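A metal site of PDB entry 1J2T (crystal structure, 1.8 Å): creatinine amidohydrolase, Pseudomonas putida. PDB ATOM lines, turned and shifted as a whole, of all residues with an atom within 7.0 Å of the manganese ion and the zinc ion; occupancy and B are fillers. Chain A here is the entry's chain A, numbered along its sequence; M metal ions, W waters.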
ATOM      1  N   GLY A  31      27.677  -3.422  17.404  1.00  0.00           N
ATOM      2  CA  GLY A  31      26.888  -2.747  16.404  1.00  0.00           C
ATOM      3  C   GLY A  31      25.418  -2.501  16.701  1.00  0.00           C
ATOM      4  O   GLY A  31      25.047  -2.102  17.803  1.00  0.00           O
ATOM      5  N   ALA A  32      24.591  -2.707  15.672  1.00  0.00           N
ATOM      6  CA  ALA A  32      23.159  -2.434  15.729  1.00  0.00           C
ATOM      7  C   ALA A  32      22.477  -2.953  14.457  1.00  0.00           C
ATOM      8  O   ALA A  32      23.125  -3.187  13.443  1.00  0.00           O
ATOM      9  CB  ALA A  32      22.887  -0.922  15.858  1.00  0.00           C
ATOM     10  N   GLU A  34      19.706  -1.437  12.219  1.00  0.00           N
ATOM     11  CA  GLU A  34      19.146  -0.108  12.159  1.00  0.00           C
ATOM     12  C   GLU A  34      18.974   0.371  10.728  1.00  0.00           C
ATOM     13  O   GLU A  34      19.796   0.113   9.867  1.00  0.00           O
ATOM     14  CB  GLU A  34      20.088   0.860  12.913  1.00  0.00           C
ATOM     15  CG  GLU A  34      19.673   2.331  12.913  1.00  0.00           C
ATOM     16  CD  GLU A  34      20.774   3.214  13.485  1.00  0.00           C
ATOM     17  OE1 GLU A  34      20.465   4.093  14.295  1.00  0.00           O
ATOM     18  OE2 GLU A  34      21.947   3.012  13.127  1.00  0.00           O
ATOM     19  N   GLN A  35      17.872   1.065  10.478  1.00  0.00           N
ATOM     20  CA  GLN A  35      17.634   1.636   9.167  1.00  0.00           C
ATOM     21  C   GLN A  35      18.814   2.521   8.766  1.00  0.00           C
ATOM     22  O   GLN A  35      19.372   3.279   9.585  1.00  0.00           O
ATOM     23  CB  GLN A  35      16.337   2.472   9.183  1.00  0.00           C
ATOM     24  CG  GLN A  35      16.391   3.788  10.028  1.00  0.00           C
ATOM     25  CD  GLN A  35      17.040   4.972   9.295  1.00  0.00           C
ATOM     26  OE1 GLN A  35      17.127   4.983   8.070  1.00  0.00           O
ATOM     27  NE2 GLN A  35      17.460   5.995  10.063  1.00  0.00           N
ATOM     28  N   HIS A  36      19.178   2.444   7.485  1.00  0.00           N
ATOM     29  CA  HIS A  36      20.231   3.273   6.916  1.00  0.00           C
ATOM     30  C   HIS A  36      19.805   3.821   5.542  1.00  0.00           C
ATOM     31  O   HIS A  36      20.514   3.679   4.530  1.00  0.00           O
ATOM     32  CB  HIS A  36      21.521   2.466   6.789  1.00  0.00           C
ATOM     33  CG  HIS A  36      22.323   2.419   8.045  1.00  0.00           C
ATOM     34  ND1 HIS A  36      22.012   1.591   9.108  1.00  0.00           N
ATOM     35  CD2 HIS A  36      23.441   3.094   8.411  1.00  0.00           C
ATOM     36  CE1 HIS A  36      22.894   1.768  10.069  1.00  0.00           C
ATOM     37  NE2 HIS A  36      23.779   2.667   9.667  1.00  0.00           N
ATOM     38  N   MET A  40      20.869   1.597   1.430  1.00  0.00           N
ATOM     39  CA  MET A  40      21.792   0.717   2.115  1.00  0.00           C
ATOM     40  C   MET A  40      21.040  -0.197   3.072  1.00  0.00           C
ATOM     41  O   MET A  40      19.976   0.159   3.547  1.00  0.00           O
ATOM     42  CB  MET A  40      22.756   1.569   2.947  1.00  0.00           C
ATOM     43  CG  MET A  40      24.099   1.000   3.127  1.00  0.00           C
ATOM     44  SD  MET A  40      25.298   2.255   3.440  1.00  0.00           S
ATOM     45  CE  MET A  40      24.341   3.474   4.465  1.00  0.00           C
ATOM     46  N   VAL A  44      24.706  -2.456   8.695  1.00  0.00           N
ATOM     47  CA  VAL A  44      25.911  -1.639   8.512  1.00  0.00           C
ATOM     48  C   VAL A  44      26.765  -1.503   9.774  1.00  0.00           C
ATOM     49  O   VAL A  44      27.988  -1.691   9.734  1.00  0.00           O
ATOM     50  CB  VAL A  44      25.525  -0.239   7.955  1.00  0.00           C
ATOM     51  CG1 VAL A  44      26.708   0.766   8.083  1.00  0.00           C
ATOM     52  CG2 VAL A  44      25.060  -0.351   6.505  1.00  0.00           C
ATOM     53  N   ASP A  45      26.116  -1.219  10.901  1.00  0.00           N
ATOM     54  CA  ASP A  45      26.851  -0.941  12.145  1.00  0.00           C
ATOM     55  C   ASP A  45      27.546  -2.166  12.730  1.00  0.00           C
ATOM     56  O   ASP A  45      28.374  -2.022  13.629  1.00  0.00           O
ATOM     57  CB  ASP A  45      25.951  -0.294  13.212  1.00  0.00           C
ATOM     58  CG  ASP A  45      25.495   1.120  12.838  1.00  0.00           C
ATOM     59  OD1 ASP A  45      25.888   1.652  11.752  1.00  0.00           O
ATOM     60  OD2 ASP A  45      24.757   1.793  13.599  1.00  0.00           O
ATOM     61  N   LEU A  48      30.655  -2.924   9.469  1.00  0.00           N
ATOM     62  CA  LEU A  48      31.788  -2.009   9.365  1.00  0.00           C
ATOM     63  C   LEU A  48      32.840  -2.186  10.470  1.00  0.00           C
ATOM     64  O   LEU A  48      34.013  -2.436  10.150  1.00  0.00           O
ATOM     65  CB  LEU A  48      31.289  -0.560   9.245  1.00  0.00           C
ATOM     66  CG  LEU A  48      30.519  -0.323   7.928  1.00  0.00           C
ATOM     67  CD1 LEU A  48      30.152   1.140   7.741  1.00  0.00           C
ATOM     68  CD2 LEU A  48      31.261  -0.848   6.681  1.00  0.00           C
ATOM     69  N   TYR A  72      21.801  -0.070  21.248  1.00  0.00           N
ATOM     70  CA  TYR A  72      20.885   0.833  21.922  1.00  0.00           C
ATOM     71  C   TYR A  72      19.961   1.550  20.931  1.00  0.00           C
ATOM     72  O   TYR A  72      20.272   1.680  19.732  1.00  0.00           O
ATOM     73  CB  TYR A  72      21.628   1.834  22.822  1.00  0.00           C
ATOM     74  CG  TYR A  72      20.643   2.631  23.659  1.00  0.00           C
ATOM     75  CD1 TYR A  72      19.849   1.994  24.603  1.00  0.00           C
ATOM     76  CD2 TYR A  72      20.445   3.986  23.437  1.00  0.00           C
ATOM     77  CE1 TYR A  72      18.910   2.714  25.346  1.00  0.00           C
ATOM     78  CE2 TYR A  72      19.526   4.696  24.162  1.00  0.00           C
ATOM     79  CZ  TYR A  72      18.753   4.054  25.109  1.00  0.00           C
ATOM     80  OH  TYR A  72      17.820   4.766  25.807  1.00  0.00           O
ATOM     81  N   SER A  74      18.054   3.861  18.604  1.00  0.00           N
ATOM     82  CA  SER A  74      18.390   4.936  17.702  1.00  0.00           C
ATOM     83  C   SER A  74      17.822   6.264  18.218  1.00  0.00           C
ATOM     84  O   SER A  74      16.664   6.322  18.651  1.00  0.00           O
ATOM     85  CB  SER A  74      17.833   4.616  16.307  1.00  0.00           C
ATOM     86  OG  SER A  74      17.987   5.713  15.432  1.00  0.00           O
ATOM     87  N   SER A  78      21.066  11.401  15.940  1.00  0.00           N
ATOM     88  CA  SER A  78      22.224  10.583  15.572  1.00  0.00           C
ATOM     89  C   SER A  78      21.969   9.301  14.759  1.00  0.00           C
ATOM     90  O   SER A  78      22.914   8.660  14.298  1.00  0.00           O
ATOM     91  CB  SER A  78      23.022  10.213  16.828  1.00  0.00           C
ATOM     92  OG  SER A  78      22.163   9.658  17.811  1.00  0.00           O
ATOM     93  N   GLY A  79      20.702   8.910  14.582  1.00  0.00           N
ATOM     94  CA  GLY A  79      20.375   7.700  13.830  1.00  0.00           C
ATOM     95  C   GLY A  79      18.989   7.665  13.186  1.00  0.00           C
ATOM     96  O   GLY A  79      18.529   6.620  12.729  1.00  0.00           O
ATOM     97  N   GLY A 119      30.336   0.583  16.581  1.00  0.00           N
ATOM     98  CA  GLY A 119      29.930   0.998  15.248  1.00  0.00           C
ATOM     99  C   GLY A 119      28.604   1.726  15.184  1.00  0.00           C
ATOM    100  O   GLY A 119      28.198   2.146  14.102  1.00  0.00           O
ATOM    101  N   HIS A 120      27.921   1.870  16.322  1.00  0.00           N
ATOM    102  CA  HIS A 120      26.604   2.515  16.412  1.00  0.00           C
ATOM    103  C   HIS A 120      26.697   3.609  17.456  1.00  0.00           C
ATOM    104  O   HIS A 120      26.935   3.341  18.628  1.00  0.00           O
ATOM    105  CB  HIS A 120      25.558   1.469  16.770  1.00  0.00           C
ATOM    106  CG  HIS A 120      24.184   2.008  17.035  1.00  0.00           C
ATOM    107  ND1 HIS A 120      23.425   2.638  16.069  1.00  0.00           N
ATOM    108  CD2 HIS A 120      23.399   1.918  18.132  1.00  0.00           C
ATOM    109  CE1 HIS A 120      22.238   2.936  16.569  1.00  0.00           C
ATOM    110  NE2 HIS A 120      22.191   2.502  17.820  1.00  0.00           N
ATOM    111  N   TYR A 121      26.513   4.845  16.996  1.00  0.00           N
ATOM    112  CA  TYR A 121      26.777   6.043  17.798  1.00  0.00           C
ATOM    113  C   TYR A 121      26.189   5.990  19.203  1.00  0.00           C
ATOM    114  O   TYR A 121      26.878   6.296  20.183  1.00  0.00           O
ATOM    115  CB  TYR A 121      26.225   7.277  17.073  1.00  0.00           C
ATOM    116  CG  TYR A 121      26.719   8.586  17.626  1.00  0.00           C
ATOM    117  CD1 TYR A 121      27.851   9.203  17.093  1.00  0.00           C
ATOM    118  CD2 TYR A 121      26.075   9.207  18.690  1.00  0.00           C
ATOM    119  CE1 TYR A 121      28.308  10.401  17.581  1.00  0.00           C
ATOM    120  CE2 TYR A 121      26.544  10.411  19.199  1.00  0.00           C
ATOM    121  CZ  TYR A 121      27.665  11.003  18.636  1.00  0.00           C
ATOM    122  OH  TYR A 121      28.160  12.207  19.105  1.00  0.00           O
ATOM    123  N   GLU A 122      24.943   5.532  19.295  1.00  0.00           N
ATOM    124  CA  GLU A 122      24.191   5.518  20.547  1.00  0.00           C
ATOM    125  C   GLU A 122      24.666   4.516  21.590  1.00  0.00           C
ATOM    126  O   GLU A 122      24.283   4.621  22.746  1.00  0.00           O
ATOM    127  CB  GLU A 122      22.712   5.233  20.232  1.00  0.00           C
ATOM    128  CG  GLU A 122      21.983   6.380  19.557  1.00  0.00           C
ATOM    129  CD  GLU A 122      22.157   6.399  18.055  1.00  0.00           C
ATOM    130  OE1 GLU A 122      23.060   5.711  17.544  1.00  0.00           O
ATOM    131  OE2 GLU A 122      21.403   7.129  17.380  1.00  0.00           O
ATOM    132  N   TYR A 153      35.098   3.639  15.762  1.00  0.00           N
ATOM    133  CA  TYR A 153      36.113   3.610  14.699  1.00  0.00           C
ATOM    134  C   TYR A 153      36.233   4.917  13.903  1.00  0.00           C
ATOM    135  O   TYR A 153      37.347   5.289  13.489  1.00  0.00           O
ATOM    136  CB  TYR A 153      35.969   2.382  13.776  1.00  0.00           C
ATOM    137  CG  TYR A 153      34.765   2.425  12.870  1.00  0.00           C
ATOM    138  CD1 TYR A 153      34.850   2.945  11.588  1.00  0.00           C
ATOM    139  CD2 TYR A 153      33.522   1.967  13.307  1.00  0.00           C
ATOM    140  CE1 TYR A 153      33.775   3.012  10.761  1.00  0.00           C
ATOM    141  CE2 TYR A 153      32.404   2.045  12.473  1.00  0.00           C
ATOM    142  CZ  TYR A 153      32.540   2.569  11.198  1.00  0.00           C
ATOM    143  OH  TYR A 153      31.462   2.658  10.367  1.00  0.00           O
ATOM    144  N   TRP A 154      35.127   5.631  13.713  1.00  0.00           N
ATOM    145  CA  TRP A 154      35.167   6.883  12.951  1.00  0.00           C
ATOM    146  C   TRP A 154      35.993   7.979  13.620  1.00  0.00           C
ATOM    147  O   TRP A 154      36.510   8.851  12.936  1.00  0.00           O
ATOM    148  CB  TRP A 154      33.765   7.404  12.658  1.00  0.00           C
ATOM    149  CG  TRP A 154      32.910   7.529  13.868  1.00  0.00           C
ATOM    150  CD1 TRP A 154      32.917   8.523  14.791  1.00  0.00           C
ATOM    151  CD2 TRP A 154      31.945   6.575  14.304  1.00  0.00           C
ATOM    152  NE1 TRP A 154      31.984   8.270  15.768  1.00  0.00           N
ATOM    153  CE2 TRP A 154      31.370   7.073  15.488  1.00  0.00           C
ATOM    154  CE3 TRP A 154      31.475   5.364  13.787  1.00  0.00           C
ATOM    155  CZ2 TRP A 154      30.375   6.399  16.176  1.00  0.00           C
ATOM    156  CZ3 TRP A 154      30.490   4.692  14.473  1.00  0.00           C
ATOM    157  CH2 TRP A 154      29.944   5.207  15.656  1.00  0.00           C
ATOM    158  N   GLU A 177      26.301  12.252  10.928  1.00  0.00           N
ATOM    159  CA  GLU A 177      26.707  11.249   9.983  1.00  0.00           C
ATOM    160  C   GLU A 177      25.933   9.984  10.300  1.00  0.00           C
ATOM    161  O   GLU A 177      26.313   9.214  11.188  1.00  0.00           O
ATOM    162  CB  GLU A 177      28.198  10.911  10.090  1.00  0.00           C
ATOM    163  CG  GLU A 177      29.101  11.575   9.070  1.00  0.00           C
ATOM    164  CD  GLU A 177      28.585  11.504   7.654  1.00  0.00           C
ATOM    165  OE1 GLU A 177      28.144  12.568   7.174  1.00  0.00           O
ATOM    166  OE2 GLU A 177      28.635  10.408   7.013  1.00  0.00           O
ATOM    167  N   HIS A 178      24.822   9.808   9.615  1.00  0.00           N
ATOM    168  CA  HIS A 178      24.108   8.544   9.687  1.00  0.00           C
ATOM    169  C   HIS A 178      23.629   8.239   8.275  1.00  0.00           C
ATOM    170  O   HIS A 178      22.812   8.954   7.729  1.00  0.00           O
ATOM    171  CB  HIS A 178      22.929   8.582  10.659  1.00  0.00           C
ATOM    172  CG  HIS A 178      22.107   7.330  10.611  1.00  0.00           C
ATOM    173  ND1 HIS A 178      22.604   6.106  10.986  1.00  0.00           N
ATOM    174  CD2 HIS A 178      20.841   7.107  10.186  1.00  0.00           C
ATOM    175  CE1 HIS A 178      21.677   5.184  10.795  1.00  0.00           C
ATOM    176  NE2 HIS A 178      20.599   5.765  10.313  1.00  0.00           N
ATOM    177  N   GLY A 179      24.180   7.169   7.697  1.00  0.00           N
ATOM    178  CA  GLY A 179      23.827   6.731   6.361  1.00  0.00           C
ATOM    179  C   GLY A 179      24.307   7.677   5.288  1.00  0.00           C
ATOM    180  O   GLY A 179      23.833   7.639   4.150  1.00  0.00           O
ATOM    181  N   GLU A 183      29.670   6.182   5.991  1.00  0.00           N
ATOM    182  CA  GLU A 183      29.268   4.776   5.997  1.00  0.00           C
ATOM    183  C   GLU A 183      29.029   4.242   4.605  1.00  0.00           C
ATOM    184  O   GLU A 183      29.390   3.104   4.304  1.00  0.00           O
ATOM    185  CB  GLU A 183      28.007   4.580   6.839  1.00  0.00           C
ATOM    186  CG  GLU A 183      28.228   4.816   8.315  1.00  0.00           C
ATOM    187  CD  GLU A 183      26.970   4.566   9.136  1.00  0.00           C
ATOM    188  OE1 GLU A 183      27.047   3.741  10.067  1.00  0.00           O
ATOM    189  OE2 GLU A 183      25.922   5.172   8.825  1.00  0.00           O
HETATM  190 MN    MN M   1      23.738   3.513  14.013  1.00  0.00          MN
HETATM  191 ZN    ZN M   2      25.300   3.323  10.887  1.00  0.00          ZN
HETATM  192  O   HOH W   1      24.660   4.457  12.260  1.00  0.00           O
HETATM  193  O   HOH W   2      26.585   4.937  14.037  1.00  0.00           O
HETATM  194  O   HOH W   3      23.609   5.483  14.870  1.00  0.00           O
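A ring nitrogen (NE2) of His 120 sits close to the side-chain carboxylate of Glu 122 (3.3 Å).
The backbone carbonyl oxygen of Glu 34 lies within hydrogen-bond range of a ring nitrogen (ND1) of His 36 (2.8 Å).
The side-chain hydroxyl (OG) of Ser 74 lies within hydrogen-bond range of the side-chain carboxylate (OE1) of Glu 34 (3.2 Å).
The backbone carbonyl oxygen of Gln 35 lies within hydrogen-bond range of a ring nitrogen (NE2) of His 178.
A ring nitrogen (NE2) of His 120 lies within hydrogen-bond range of the backbone carbonyl oxygen of Tyr 72, at 2.8 Å.
OE2 of Glu 183 sits at hydrogen-bond distance from N of Gly 179 (2.9 Å).
The backbone carbonyl oxygen (O) of Gly 79 sits at hydrogen-bond distance from a ring nitrogen (NE2) of His 178 (3.3 Å).
Within 4 Å of the manganese ion: Glu 34, Asp 45 and His 120.
Merely in contact with the zinc ion: His 178.
Four residues have an atom within 4 Å of the zinc ion: His 36, Asp 45, His 178 and Glu 183.
The nearest printed residue that does not touch the zinc ion is Glu 34 (4.04 Å).
The manganese ion is bound by the side-chain carboxylate (OD2) of Asp 45 (2.0 Å), the side-chain carboxylate (OE2) of Glu 34 (2.1 Å), water W3 (2.2 Å), water W1 (2.2 Å) and a ring nitrogen (ND1) of His 120 (2.3 Å).
The manganese ion has five donor atoms within binding distance.
The zinc ion is bound by water W1 (1.9 Å).
The zinc ion is bound by OD1 of Asp 45 (2.0 Å).
OE1 of Glu 183 is bound to the zinc ion.
NE2 of His 36 is bound to the zinc ion (2.1 Å).
Slightly farther from the zinc ion lies OE2 of Glu 183 (2.8 Å).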
